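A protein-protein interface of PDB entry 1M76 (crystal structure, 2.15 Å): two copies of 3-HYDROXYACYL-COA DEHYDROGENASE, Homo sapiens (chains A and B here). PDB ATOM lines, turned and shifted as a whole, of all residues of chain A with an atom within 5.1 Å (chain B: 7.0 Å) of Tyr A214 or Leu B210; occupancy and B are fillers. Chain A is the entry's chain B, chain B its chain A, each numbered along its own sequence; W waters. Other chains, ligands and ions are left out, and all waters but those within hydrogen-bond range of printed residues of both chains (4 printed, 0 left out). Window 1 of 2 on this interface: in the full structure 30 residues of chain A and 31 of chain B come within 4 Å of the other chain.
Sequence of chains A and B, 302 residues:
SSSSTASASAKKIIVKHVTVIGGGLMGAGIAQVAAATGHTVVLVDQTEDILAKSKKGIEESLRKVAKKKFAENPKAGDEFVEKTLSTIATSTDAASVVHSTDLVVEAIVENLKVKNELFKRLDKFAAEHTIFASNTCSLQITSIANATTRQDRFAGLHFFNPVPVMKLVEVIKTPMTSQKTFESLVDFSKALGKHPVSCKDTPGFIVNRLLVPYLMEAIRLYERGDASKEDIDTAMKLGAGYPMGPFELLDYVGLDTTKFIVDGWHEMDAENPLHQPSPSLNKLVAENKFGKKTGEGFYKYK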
ATOM      1  N   LEU A 210      -8.011  -2.467  28.411  1.00  0.00           N
ATOM      2  CA  LEU A 210      -7.161  -3.494  27.804  1.00  0.00           C
ATOM      3  C   LEU A 210      -7.925  -4.716  27.284  1.00  0.00           C
ATOM      4  O   LEU A 210      -7.573  -5.285  26.252  1.00  0.00           O
ATOM      5  CB  LEU A 210      -6.116  -3.970  28.812  1.00  0.00           C
ATOM      6  CG  LEU A 210      -5.172  -2.937  29.432  1.00  0.00           C
ATOM      7  CD1 LEU A 210      -4.243  -3.655  30.409  1.00  0.00           C
ATOM      8  CD2 LEU A 210      -4.367  -2.225  28.344  1.00  0.00           C
ATOM      9  N   LEU A 211      -8.971  -5.114  28.001  1.00  0.00           N
ATOM     10  CA  LEU A 211      -9.753  -6.292  27.629  1.00  0.00           C
ATOM     11  C   LEU A 211     -10.682  -6.097  26.448  1.00  0.00           C
ATOM     12  O   LEU A 211     -10.664  -6.888  25.504  1.00  0.00           O
ATOM     13  CB  LEU A 211     -10.573  -6.777  28.835  1.00  0.00           C
ATOM     14  CG  LEU A 211     -11.449  -8.022  28.659  1.00  0.00           C
ATOM     15  CD1 LEU A 211     -10.571  -9.271  28.532  1.00  0.00           C
ATOM     16  CD2 LEU A 211     -12.390  -8.156  29.856  1.00  0.00           C
ATOM     17  N   VAL A 212     -11.504  -5.051  26.492  1.00  0.00           N
ATOM     18  CA  VAL A 212     -12.460  -4.834  25.419  1.00  0.00           C
ATOM     19  C   VAL A 212     -11.838  -4.697  24.037  1.00  0.00           C
ATOM     20  O   VAL A 212     -12.336  -5.281  23.074  1.00  0.00           O
ATOM     21  CB  VAL A 212     -13.390  -3.628  25.731  1.00  0.00           C
ATOM     22  CG1 VAL A 212     -14.294  -3.329  24.535  1.00  0.00           C
ATOM     23  CG2 VAL A 212     -14.254  -3.957  26.951  1.00  0.00           C
ATOM     24  N   PRO A 213     -10.742  -3.932  23.903  1.00  0.00           N
ATOM     25  CA  PRO A 213     -10.180  -3.841  22.550  1.00  0.00           C
ATOM     26  C   PRO A 213      -9.706  -5.216  22.054  1.00  0.00           C
ATOM     27  O   PRO A 213      -9.764  -5.519  20.858  1.00  0.00           O
ATOM     28  CB  PRO A 213      -9.035  -2.845  22.723  1.00  0.00           C
ATOM     29  CG  PRO A 213      -9.559  -1.945  23.813  1.00  0.00           C
ATOM     30  CD  PRO A 213     -10.104  -2.956  24.800  1.00  0.00           C
ATOM     31  N   TYR A 214      -9.238  -6.039  22.986  1.00  0.00           N
ATOM     32  CA  TYR A 214      -8.776  -7.387  22.665  1.00  0.00           C
ATOM     33  C   TYR A 214      -9.972  -8.225  22.191  1.00  0.00           C
ATOM     34  O   TYR A 214      -9.885  -8.945  21.197  1.00  0.00           O
ATOM     35  CB  TYR A 214      -8.141  -8.014  23.910  1.00  0.00           C
ATOM     36  CG  TYR A 214      -8.331  -9.511  24.033  1.00  0.00           C
ATOM     37  CD1 TYR A 214      -7.733 -10.391  23.135  1.00  0.00           C
ATOM     38  CD2 TYR A 214      -9.122 -10.045  25.053  1.00  0.00           C
ATOM     39  CE1 TYR A 214      -7.917 -11.777  23.248  1.00  0.00           C
ATOM     40  CE2 TYR A 214      -9.313 -11.425  25.176  1.00  0.00           C
ATOM     41  CZ  TYR A 214      -8.707 -12.283  24.272  1.00  0.00           C
ATOM     42  OH  TYR A 214      -8.886 -13.646  24.399  1.00  0.00           O
ATOM     43  N   LEU A 215     -11.092  -8.122  22.904  1.00  0.00           N
ATOM     44  CA  LEU A 215     -12.289  -8.871  22.526  1.00  0.00           C
ATOM     45  C   LEU A 215     -12.742  -8.472  21.124  1.00  0.00           C
ATOM     46  O   LEU A 215     -13.134  -9.327  20.331  1.00  0.00           O
ATOM     47  CB  LEU A 215     -13.418  -8.635  23.536  1.00  0.00           C
ATOM     48  CG  LEU A 215     -13.188  -9.247  24.919  1.00  0.00           C
ATOM     49  CD1 LEU A 215     -14.305  -8.817  25.856  1.00  0.00           C
ATOM     50  CD2 LEU A 215     -13.127 -10.770  24.822  1.00  0.00           C
ATOM     51  N   MET A 216     -12.682  -7.177  20.815  1.00  0.00           N
ATOM     52  CA  MET A 216     -13.075  -6.699  19.490  1.00  0.00           C
ATOM     53  C   MET A 216     -12.145  -7.281  18.428  1.00  0.00           C
ATOM     54  O   MET A 216     -12.588  -7.670  17.347  1.00  0.00           O
ATOM     55  CB  MET A 216     -13.031  -5.162  19.416  1.00  0.00           C
ATOM     56  CG  MET A 216     -14.135  -4.437  20.203  1.00  0.00           C
ATOM     57  SD  MET A 216     -15.844  -4.980  19.847  1.00  0.00           S
ATOM     58  CE  MET A 216     -16.020  -4.468  18.160  1.00  0.00           C
ATOM     59  N   GLU A 217     -10.848  -7.330  18.725  1.00  0.00           N
ATOM     60  CA  GLU A 217      -9.896  -7.883  17.763  1.00  0.00           C
ATOM     61  C   GLU A 217     -10.226  -9.352  17.500  1.00  0.00           C
ATOM     62  O   GLU A 217     -10.112  -9.831  16.374  1.00  0.00           O
ATOM     63  CB  GLU A 217      -8.461  -7.736  18.280  1.00  0.00           C
ATOM     64  CG  GLU A 217      -7.825  -6.381  17.956  1.00  0.00           C
ATOM     65  CD  GLU A 217      -7.733  -6.122  16.458  1.00  0.00           C
ATOM     66  OE1 GLU A 217      -8.768  -5.799  15.836  1.00  0.00           O
ATOM     67  OE2 GLU A 217      -6.631  -6.250  15.890  1.00  0.00           O
ATOM     68  N   ALA A 218     -10.646 -10.063  18.541  1.00  0.00           N
ATOM     69  CA  ALA A 218     -11.014 -11.465  18.386  1.00  0.00           C
ATOM     70  C   ALA A 218     -12.159 -11.517  17.382  1.00  0.00           C
ATOM     71  O   ALA A 218     -12.141 -12.316  16.450  1.00  0.00           O
ATOM     72  CB  ALA A 218     -11.455 -12.052  19.719  1.00  0.00           C
ATOM     73  N   LEU A 221     -10.956 -10.733  13.797  1.00  0.00           N
ATOM     74  CA  LEU A 221     -10.200 -11.842  13.224  1.00  0.00           C
ATOM     75  C   LEU A 221     -11.193 -12.867  12.658  1.00  0.00           C
ATOM     76  O   LEU A 221     -10.996 -13.408  11.567  1.00  0.00           O
ATOM     77  CB  LEU A 221      -9.321 -12.484  14.298  1.00  0.00           C
ATOM     78  CG  LEU A 221      -8.347 -13.597  13.892  1.00  0.00           C
ATOM     79  CD1 LEU A 221      -7.310 -13.771  14.983  1.00  0.00           C
ATOM     80  CD2 LEU A 221      -9.088 -14.894  13.662  1.00  0.00           C
ATOM     81  N   ILE A 232     -10.667 -20.070  17.813  1.00  0.00           N
ATOM     82  CA  ILE A 232     -10.118 -18.900  18.490  1.00  0.00           C
ATOM     83  C   ILE A 232     -10.268 -19.084  20.001  1.00  0.00           C
ATOM     84  O   ILE A 232      -9.340 -18.810  20.763  1.00  0.00           O
ATOM     85  CB  ILE A 232     -10.832 -17.594  18.055  1.00  0.00           C
ATOM     86  CG1 ILE A 232     -10.477 -17.274  16.599  1.00  0.00           C
ATOM     87  CG2 ILE A 232     -10.393 -16.438  18.945  1.00  0.00           C
ATOM     88  CD1 ILE A 232     -11.375 -16.239  15.939  1.00  0.00           C
ATOM     89  N   MET A 236      -6.997 -19.464  22.651  1.00  0.00           N
ATOM     90  CA  MET A 236      -6.737 -18.550  23.758  1.00  0.00           C
ATOM     91  C   MET A 236      -6.724 -19.245  25.121  1.00  0.00           C
ATOM     92  O   MET A 236      -5.951 -18.877  26.004  1.00  0.00           O
ATOM     93  CB  MET A 236      -7.757 -17.412  23.755  1.00  0.00           C
ATOM     94  CG  MET A 236      -7.714 -16.549  22.492  1.00  0.00           C
ATOM     95  SD  MET A 236      -6.044 -15.945  22.085  1.00  0.00           S
ATOM     96  CE  MET A 236      -5.668 -14.942  23.540  1.00  0.00           C
ATOM     97  N   TYR A 242      -6.197 -18.680  29.332  1.00  0.00           N
ATOM     98  CA  TYR A 242      -7.343 -17.878  29.761  1.00  0.00           C
ATOM     99  C   TYR A 242      -8.497 -18.755  30.224  1.00  0.00           C
ATOM    100  O   TYR A 242      -8.713 -19.833  29.680  1.00  0.00           O
ATOM    101  CB  TYR A 242      -7.826 -16.976  28.618  1.00  0.00           C
ATOM    102  CG  TYR A 242      -6.892 -15.831  28.261  1.00  0.00           C
ATOM    103  CD1 TYR A 242      -5.723 -15.592  28.988  1.00  0.00           C
ATOM    104  CD2 TYR A 242      -7.205 -14.960  27.218  1.00  0.00           C
ATOM    105  CE1 TYR A 242      -4.892 -14.505  28.685  1.00  0.00           C
ATOM    106  CE2 TYR A 242      -6.384 -13.874  26.908  1.00  0.00           C
ATOM    107  CZ  TYR A 242      -5.234 -13.653  27.643  1.00  0.00           C
ATOM    108  OH  TYR A 242      -4.434 -12.581  27.334  1.00  0.00           O
ATOM    109  N   MET A 244     -11.621 -18.210  29.836  1.00  0.00           N
ATOM    110  CA  MET A 244     -12.598 -18.258  28.754  1.00  0.00           C
ATOM    111  C   MET A 244     -12.067 -17.716  27.435  1.00  0.00           C
ATOM    112  O   MET A 244     -11.281 -16.768  27.413  1.00  0.00           O
ATOM    113  CB  MET A 244     -13.844 -17.442  29.120  1.00  0.00           C
ATOM    114  CG  MET A 244     -14.565 -17.882  30.378  1.00  0.00           C
ATOM    115  SD  MET A 244     -15.982 -16.801  30.765  1.00  0.00           S
ATOM    116  CE  MET A 244     -17.267 -18.052  31.113  1.00  0.00           C
ATOM    117  N   GLY A 245     -12.517 -18.321  26.339  1.00  0.00           N
ATOM    118  CA  GLY A 245     -12.134 -17.858  25.023  1.00  0.00           C
ATOM    119  C   GLY A 245     -12.813 -16.513  24.866  1.00  0.00           C
ATOM    120  O   GLY A 245     -13.787 -16.238  25.572  1.00  0.00           O
ATOM    121  N   PRO A 246     -12.348 -15.653  23.949  1.00  0.00           N
ATOM    122  CA  PRO A 246     -12.969 -14.338  23.770  1.00  0.00           C
ATOM    123  C   PRO A 246     -14.467 -14.354  23.463  1.00  0.00           C
ATOM    124  O   PRO A 246     -15.221 -13.523  23.975  1.00  0.00           O
ATOM    125  CB  PRO A 246     -12.139 -13.715  22.649  1.00  0.00           C
ATOM    126  CG  PRO A 246     -11.705 -14.916  21.849  1.00  0.00           C
ATOM    127  CD  PRO A 246     -11.323 -15.899  22.922  1.00  0.00           C
ATOM    128  N   PRO B 203      -0.372 -13.202   9.803  1.00  0.00           N
ATOM    129  CA  PRO B 203       0.471 -12.649  10.869  1.00  0.00           C
ATOM    130  C   PRO B 203       0.029 -12.883  12.314  1.00  0.00           C
ATOM    131  O   PRO B 203      -1.014 -12.391  12.756  1.00  0.00           O
ATOM    132  CB  PRO B 203       0.570 -11.158  10.506  1.00  0.00           C
ATOM    133  CG  PRO B 203      -0.615 -10.916   9.606  1.00  0.00           C
ATOM    134  CD  PRO B 203      -0.703 -12.174   8.800  1.00  0.00           C
ATOM    135  N   GLY B 204       0.842 -13.637  13.049  1.00  0.00           N
ATOM    136  CA  GLY B 204       0.537 -13.922  14.441  1.00  0.00           C
ATOM    137  C   GLY B 204      -0.448 -15.063  14.604  1.00  0.00           C
ATOM    138  O   GLY B 204      -0.818 -15.426  15.727  1.00  0.00           O
ATOM    139  N   PHE B 205      -0.872 -15.628  13.478  1.00  0.00           N
ATOM    140  CA  PHE B 205      -1.819 -16.734  13.484  1.00  0.00           C
ATOM    141  C   PHE B 205      -2.996 -16.359  14.380  1.00  0.00           C
ATOM    142  O   PHE B 205      -3.637 -15.328  14.146  1.00  0.00           O
ATOM    143  CB  PHE B 205      -1.105 -18.003  13.962  1.00  0.00           C
ATOM    144  CG  PHE B 205       0.248 -18.203  13.309  1.00  0.00           C
ATOM    145  CD1 PHE B 205       0.359 -18.280  11.917  1.00  0.00           C
ATOM    146  CD2 PHE B 205       1.408 -18.258  14.073  1.00  0.00           C
ATOM    147  CE1 PHE B 205       1.614 -18.404  11.301  1.00  0.00           C
ATOM    148  CE2 PHE B 205       2.667 -18.383  13.471  1.00  0.00           C
ATOM    149  CZ  PHE B 205       2.769 -18.454  12.083  1.00  0.00           C
ATOM    150  N   ILE B 206      -3.284 -17.158  15.401  1.00  0.00           N
ATOM    151  CA  ILE B 206      -4.400 -16.814  16.267  1.00  0.00           C
ATOM    152  C   ILE B 206      -3.981 -16.132  17.551  1.00  0.00           C
ATOM    153  O   ILE B 206      -4.243 -14.952  17.746  1.00  0.00           O
ATOM    154  CB  ILE B 206      -5.255 -18.040  16.672  1.00  0.00           C
ATOM    155  CG1 ILE B 206      -6.039 -18.582  15.474  1.00  0.00           C
ATOM    156  CG2 ILE B 206      -6.247 -17.631  17.760  1.00  0.00           C
ATOM    157  CD1 ILE B 206      -6.859 -19.825  15.817  1.00  0.00           C
ATOM    158  N   VAL B 207      -3.329 -16.889  18.421  1.00  0.00           N
ATOM    159  CA  VAL B 207      -2.930 -16.382  19.720  1.00  0.00           C
ATOM    160  C   VAL B 207      -2.137 -15.079  19.723  1.00  0.00           C
ATOM    161  O   VAL B 207      -2.580 -14.097  20.313  1.00  0.00           O
ATOM    162  CB  VAL B 207      -2.166 -17.464  20.505  1.00  0.00           C
ATOM    163  CG1 VAL B 207      -1.806 -16.948  21.892  1.00  0.00           C
ATOM    164  CG2 VAL B 207      -3.029 -18.719  20.613  1.00  0.00           C
ATOM    165  N   ASN B 208      -0.979 -15.054  19.071  1.00  0.00           N
ATOM    166  CA  ASN B 208      -0.174 -13.838  19.052  1.00  0.00           C
ATOM    167  C   ASN B 208      -0.870 -12.642  18.428  1.00  0.00           C
ATOM    168  O   ASN B 208      -0.771 -11.532  18.939  1.00  0.00           O
ATOM    169  CB  ASN B 208       1.159 -14.086  18.357  1.00  0.00           C
ATOM    170  CG  ASN B 208       2.080 -14.922  19.198  1.00  0.00           C
ATOM    171  OD1 ASN B 208       1.955 -14.940  20.425  1.00  0.00           O
ATOM    172  ND2 ASN B 208       3.023 -15.611  18.560  1.00  0.00           N
ATOM    173  N   ARG B 209      -1.581 -12.863  17.331  1.00  0.00           N
ATOM    174  CA  ARG B 209      -2.296 -11.778  16.678  1.00  0.00           C
ATOM    175  C   ARG B 209      -3.215 -11.059  17.677  1.00  0.00           C
ATOM    176  O   ARG B 209      -3.508  -9.872  17.521  1.00  0.00           O
ATOM    177  CB  ARG B 209      -3.124 -12.328  15.520  1.00  0.00           C
ATOM    178  CG  ARG B 209      -3.949 -11.289  14.787  1.00  0.00           C
ATOM    179  CD  ARG B 209      -3.082 -10.282  14.070  1.00  0.00           C
ATOM    180  NE  ARG B 209      -3.889  -9.264  13.405  1.00  0.00           N
ATOM    181  CZ  ARG B 209      -4.581  -8.320  14.038  1.00  0.00           C
ATOM    182  NH1 ARG B 209      -4.560  -8.256  15.364  1.00  0.00           N
ATOM    183  NH2 ARG B 209      -5.308  -7.451  13.341  1.00  0.00           N
ATOM    184  N   LEU B 210      -3.660 -11.776  18.706  1.00  0.00           N
ATOM    185  CA  LEU B 210      -4.546 -11.183  19.707  1.00  0.00           C
ATOM    186  C   LEU B 210      -3.841 -10.842  21.020  1.00  0.00           C
ATOM    187  O   LEU B 210      -4.212  -9.887  21.706  1.00  0.00           O
ATOM    188  CB  LEU B 210      -5.715 -12.132  20.001  1.00  0.00           C
ATOM    189  CG  LEU B 210      -6.609 -12.554  18.825  1.00  0.00           C
ATOM    190  CD1 LEU B 210      -7.613 -13.598  19.303  1.00  0.00           C
ATOM    191  CD2 LEU B 210      -7.329 -11.340  18.256  1.00  0.00           C
ATOM    192  N   LEU B 211      -2.821 -11.617  21.366  1.00  0.00           N
ATOM    193  CA  LEU B 211      -2.095 -11.416  22.617  1.00  0.00           C
ATOM    194  C   LEU B 211      -1.076 -10.272  22.609  1.00  0.00           C
ATOM    195  O   LEU B 211      -1.079  -9.409  23.503  1.00  0.00           O
ATOM    196  CB  LEU B 211      -1.377 -12.714  23.003  1.00  0.00           C
ATOM    197  CG  LEU B 211      -0.551 -12.696  24.294  1.00  0.00           C
ATOM    198  CD1 LEU B 211      -1.463 -12.507  25.490  1.00  0.00           C
ATOM    199  CD2 LEU B 211       0.214 -14.003  24.419  1.00  0.00           C
ATOM    200  N   VAL B 212      -0.205 -10.278  21.605  1.00  0.00           N
ATOM    201  CA  VAL B 212       0.837  -9.276  21.507  1.00  0.00           C
ATOM    202  C   VAL B 212       0.304  -7.846  21.489  1.00  0.00           C
ATOM    203  O   VAL B 212       0.784  -7.002  22.238  1.00  0.00           O
ATOM    204  CB  VAL B 212       1.734  -9.557  20.279  1.00  0.00           C
ATOM    205  CG1 VAL B 212       2.822  -8.497  20.154  1.00  0.00           C
ATOM    206  CG2 VAL B 212       2.372 -10.935  20.438  1.00  0.00           C
ATOM    207  N   PRO B 213      -0.702  -7.553  20.650  1.00  0.00           N
ATOM    208  CA  PRO B 213      -1.204  -6.173  20.652  1.00  0.00           C
ATOM    209  C   PRO B 213      -1.753  -5.769  22.019  1.00  0.00           C
ATOM    210  O   PRO B 213      -1.699  -4.601  22.398  1.00  0.00           O
ATOM    211  CB  PRO B 213      -2.276  -6.197  19.566  1.00  0.00           C
ATOM    212  CG  PRO B 213      -1.717  -7.216  18.586  1.00  0.00           C
ATOM    213  CD  PRO B 213      -1.267  -8.318  19.523  1.00  0.00           C
ATOM    214  N   TYR B 214      -2.283  -6.743  22.756  1.00  0.00           N
ATOM    215  CA  TYR B 214      -2.831  -6.488  24.082  1.00  0.00           C
ATOM    216  C   TYR B 214      -1.692  -6.142  25.040  1.00  0.00           C
ATOM    217  O   TYR B 214      -1.817  -5.243  25.866  1.00  0.00           O
ATOM    218  CB  TYR B 214      -3.601  -7.724  24.578  1.00  0.00           C
ATOM    219  CG  TYR B 214      -3.521  -7.975  26.072  1.00  0.00           C
ATOM    220  CD1 TYR B 214      -4.155  -7.130  26.979  1.00  0.00           C
ATOM    221  CD2 TYR B 214      -2.786  -9.054  26.575  1.00  0.00           C
ATOM    222  CE1 TYR B 214      -4.061  -7.346  28.344  1.00  0.00           C
ATOM    223  CE2 TYR B 214      -2.685  -9.280  27.944  1.00  0.00           C
ATOM    224  CZ  TYR B 214      -3.322  -8.421  28.822  1.00  0.00           C
ATOM    225  OH  TYR B 214      -3.204  -8.623  30.178  1.00  0.00           O
ATOM    226  N   LEU B 215      -0.581  -6.861  24.925  1.00  0.00           N
ATOM    227  CA  LEU B 215       0.563  -6.602  25.789  1.00  0.00           C
ATOM    228  C   LEU B 215       1.136  -5.219  25.492  1.00  0.00           C
ATOM    229  O   LEU B 215       1.614  -4.536  26.395  1.00  0.00           O
ATOM    230  CB  LEU B 215       1.636  -7.676  25.589  1.00  0.00           C
ATOM    231  CG  LEU B 215       1.227  -9.106  25.953  1.00  0.00           C
ATOM    232  CD1 LEU B 215       2.352 -10.072  25.592  1.00  0.00           C
ATOM    233  CD2 LEU B 215       0.896  -9.189  27.439  1.00  0.00           C
ATOM    234  N   TYR B 242      -6.635 -13.881  34.574  1.00  0.00           N
ATOM    235  CA  TYR B 242      -5.439 -14.285  33.841  1.00  0.00           C
ATOM    236  C   TYR B 242      -4.386 -14.867  34.773  1.00  0.00           C
ATOM    237  O   TYR B 242      -4.255 -14.444  35.922  1.00  0.00           O
ATOM    238  CB  TYR B 242      -4.829 -13.094  33.100  1.00  0.00           C
ATOM    239  CG  TYR B 242      -5.602 -12.616  31.891  1.00  0.00           C
ATOM    240  CD1 TYR B 242      -6.816 -13.206  31.522  1.00  0.00           C
ATOM    241  CD2 TYR B 242      -5.117 -11.573  31.111  1.00  0.00           C
ATOM    242  CE1 TYR B 242      -7.523 -12.760  30.400  1.00  0.00           C
ATOM    243  CE2 TYR B 242      -5.815 -11.121  29.993  1.00  0.00           C
ATOM    244  CZ  TYR B 242      -7.014 -11.717  29.645  1.00  0.00           C
ATOM    245  OH  TYR B 242      -7.694 -11.262  28.536  1.00  0.00           O
ATOM    246  N   TRP B 265       6.007  -6.289  12.352  1.00  0.00           N
ATOM    247  CA  TRP B 265       4.678  -5.869  11.933  1.00  0.00           C
ATOM    248  C   TRP B 265       4.660  -4.374  11.641  1.00  0.00           C
ATOM    249  O   TRP B 265       3.942  -3.914  10.754  1.00  0.00           O
ATOM    250  CB  TRP B 265       3.639  -6.203  13.008  1.00  0.00           C
ATOM    251  CG  TRP B 265       3.408  -7.680  13.167  1.00  0.00           C
ATOM    252  CD1 TRP B 265       3.779  -8.669  12.296  1.00  0.00           C
ATOM    253  CD2 TRP B 265       2.741  -8.331  14.250  1.00  0.00           C
ATOM    254  NE1 TRP B 265       3.385  -9.893  12.772  1.00  0.00           N
ATOM    255  CE2 TRP B 265       2.744  -9.717  13.970  1.00  0.00           C
ATOM    256  CE3 TRP B 265       2.137  -7.880  15.431  1.00  0.00           C
ATOM    257  CZ2 TRP B 265       2.171 -10.658  14.832  1.00  0.00           C
ATOM    258  CZ3 TRP B 265       1.565  -8.819  16.291  1.00  0.00           C
ATOM    259  CH2 TRP B 265       1.587 -10.191  15.984  1.00  0.00           C
HETATM  260  O   HOH W   1      -7.883  -6.092  13.003  1.00  0.00           O
HETATM  261  O   HOH W   2      -7.929  -9.036  14.534  1.00  0.00           O
HETATM  262  O   HOH W   3      -5.205  -7.777  18.470  1.00  0.00           O
HETATM  263  O   HOH W   4      -6.293  -9.980  26.438  1.00  0.00           O
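Among the printed residues, merely in contact across the chains: Tyr A242 with Tyr B242 (3.3 Å), Tyr A242 with Leu B211 (3.5 Å), Leu A211 with Tyr B242 (3.5 Å), Ala A218 with Leu B210 (3.6 Å), Glu A217 with Leu B210 (3.6 Å), Tyr A214 with Tyr B242 (3.7 Å), Tyr A242 with Tyr B214 (3.8 Å), Tyr A214 with Leu B210 (3.8 Å), Met A236 with Val B207 (3.9 Å), Leu A210 with Tyr B214 (3.95 Å), Met A236 with Leu B210 (3.96 Å) and Ile A232 with Leu B210 (3.99 Å).
Water W4 bridges OH of Tyr B242 and OH of Tyr A242.
Water W3 bridges the backbone carbonyl oxygen of Arg B209 (2.9 Å) and the side-chain carboxylate of Glu A217 (3.3 Å).
Water W1 bridges NH2 of Arg B209 and OE1 of Glu A217.
Water W2 lies within hydrogen-bond range of O of Glu A217 (3.0 Å) and NH2 of Arg B209 (3.3 Å).
Leu A210 touches Tyr B214, and with the chains exchanged Tyr A214 touches Leu B210.
Leu A211 touches Tyr B242, and with the chains exchanged Tyr A242 touches Leu B211.
Tyr A214 touches Tyr B242, and with the chains exchanged Tyr A242 touches Tyr B214.
Tyr B242 touches its own counterpart, Tyr A242.
Positions printed for both chains: 210, 211, 212, 213, 214, 215 and 242.
Of the 15 printed residues of chain B, 6 touch a printed residue of chain A.
Hydrophobic or aromatic side chains of chain B that line the printed part of chain A: Leu B210, Leu B211, Tyr B214 and Tyr B242.
Among the printed residues, 13 pairs touch across the chains.
Among the printed residues, Asp or Glu carboxylates within 4 Å of a Lys or Arg side-chain nitrogen of the other chain: Glu A217 with Arg B209 (2.9 Å).
NH1 of Arg B209 is in salt-bridge range of OE2 of Glu A217, 2.9 Å away.
The backbone NH (N) of Arg B209 is in hydrogen-bond range of the backbone carbonyl oxygen (O) of Gly B204 (3.1 Å).
The backbone carbonyl oxygen (O) of Met A236 is in hydrogen-bond range of the backbone NH (N) of Tyr A242, at 3.3 Å.
Printed residues of chain B within 4 Å of Leu A210: Tyr B214 (3.95 Å).
Of chain B, only Leu B210 (3.8 Å) and Tyr B242 (3.7 Å) come within 4 Å of Tyr A214.
Of the printed residues of chain B, Ile A232 touches Leu B210 (3.99 Å).
Of the printed residues of chain A, Val B207 touches Met A236.
Printed residues of chain A within 4 Å of Leu B210: Tyr A214 (3.8 Å), Glu A217 (3.6 Å), Ala A218 (3.6 Å), Ile A232 (3.99 Å) and Met A236 (3.96 Å).
Printed residues of chain A within 4 Å of Tyr B242: Leu A211 (3.5 Å), Tyr A214 (3.7 Å) and Tyr A242 (3.3 Å).
The nearest residue of chain B that does not touch Tyr A214 is Tyr B214 (4.6 Å).
The nearest printed residue of chain A that does not touch Arg B209 is Leu A221 (4.2 Å).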
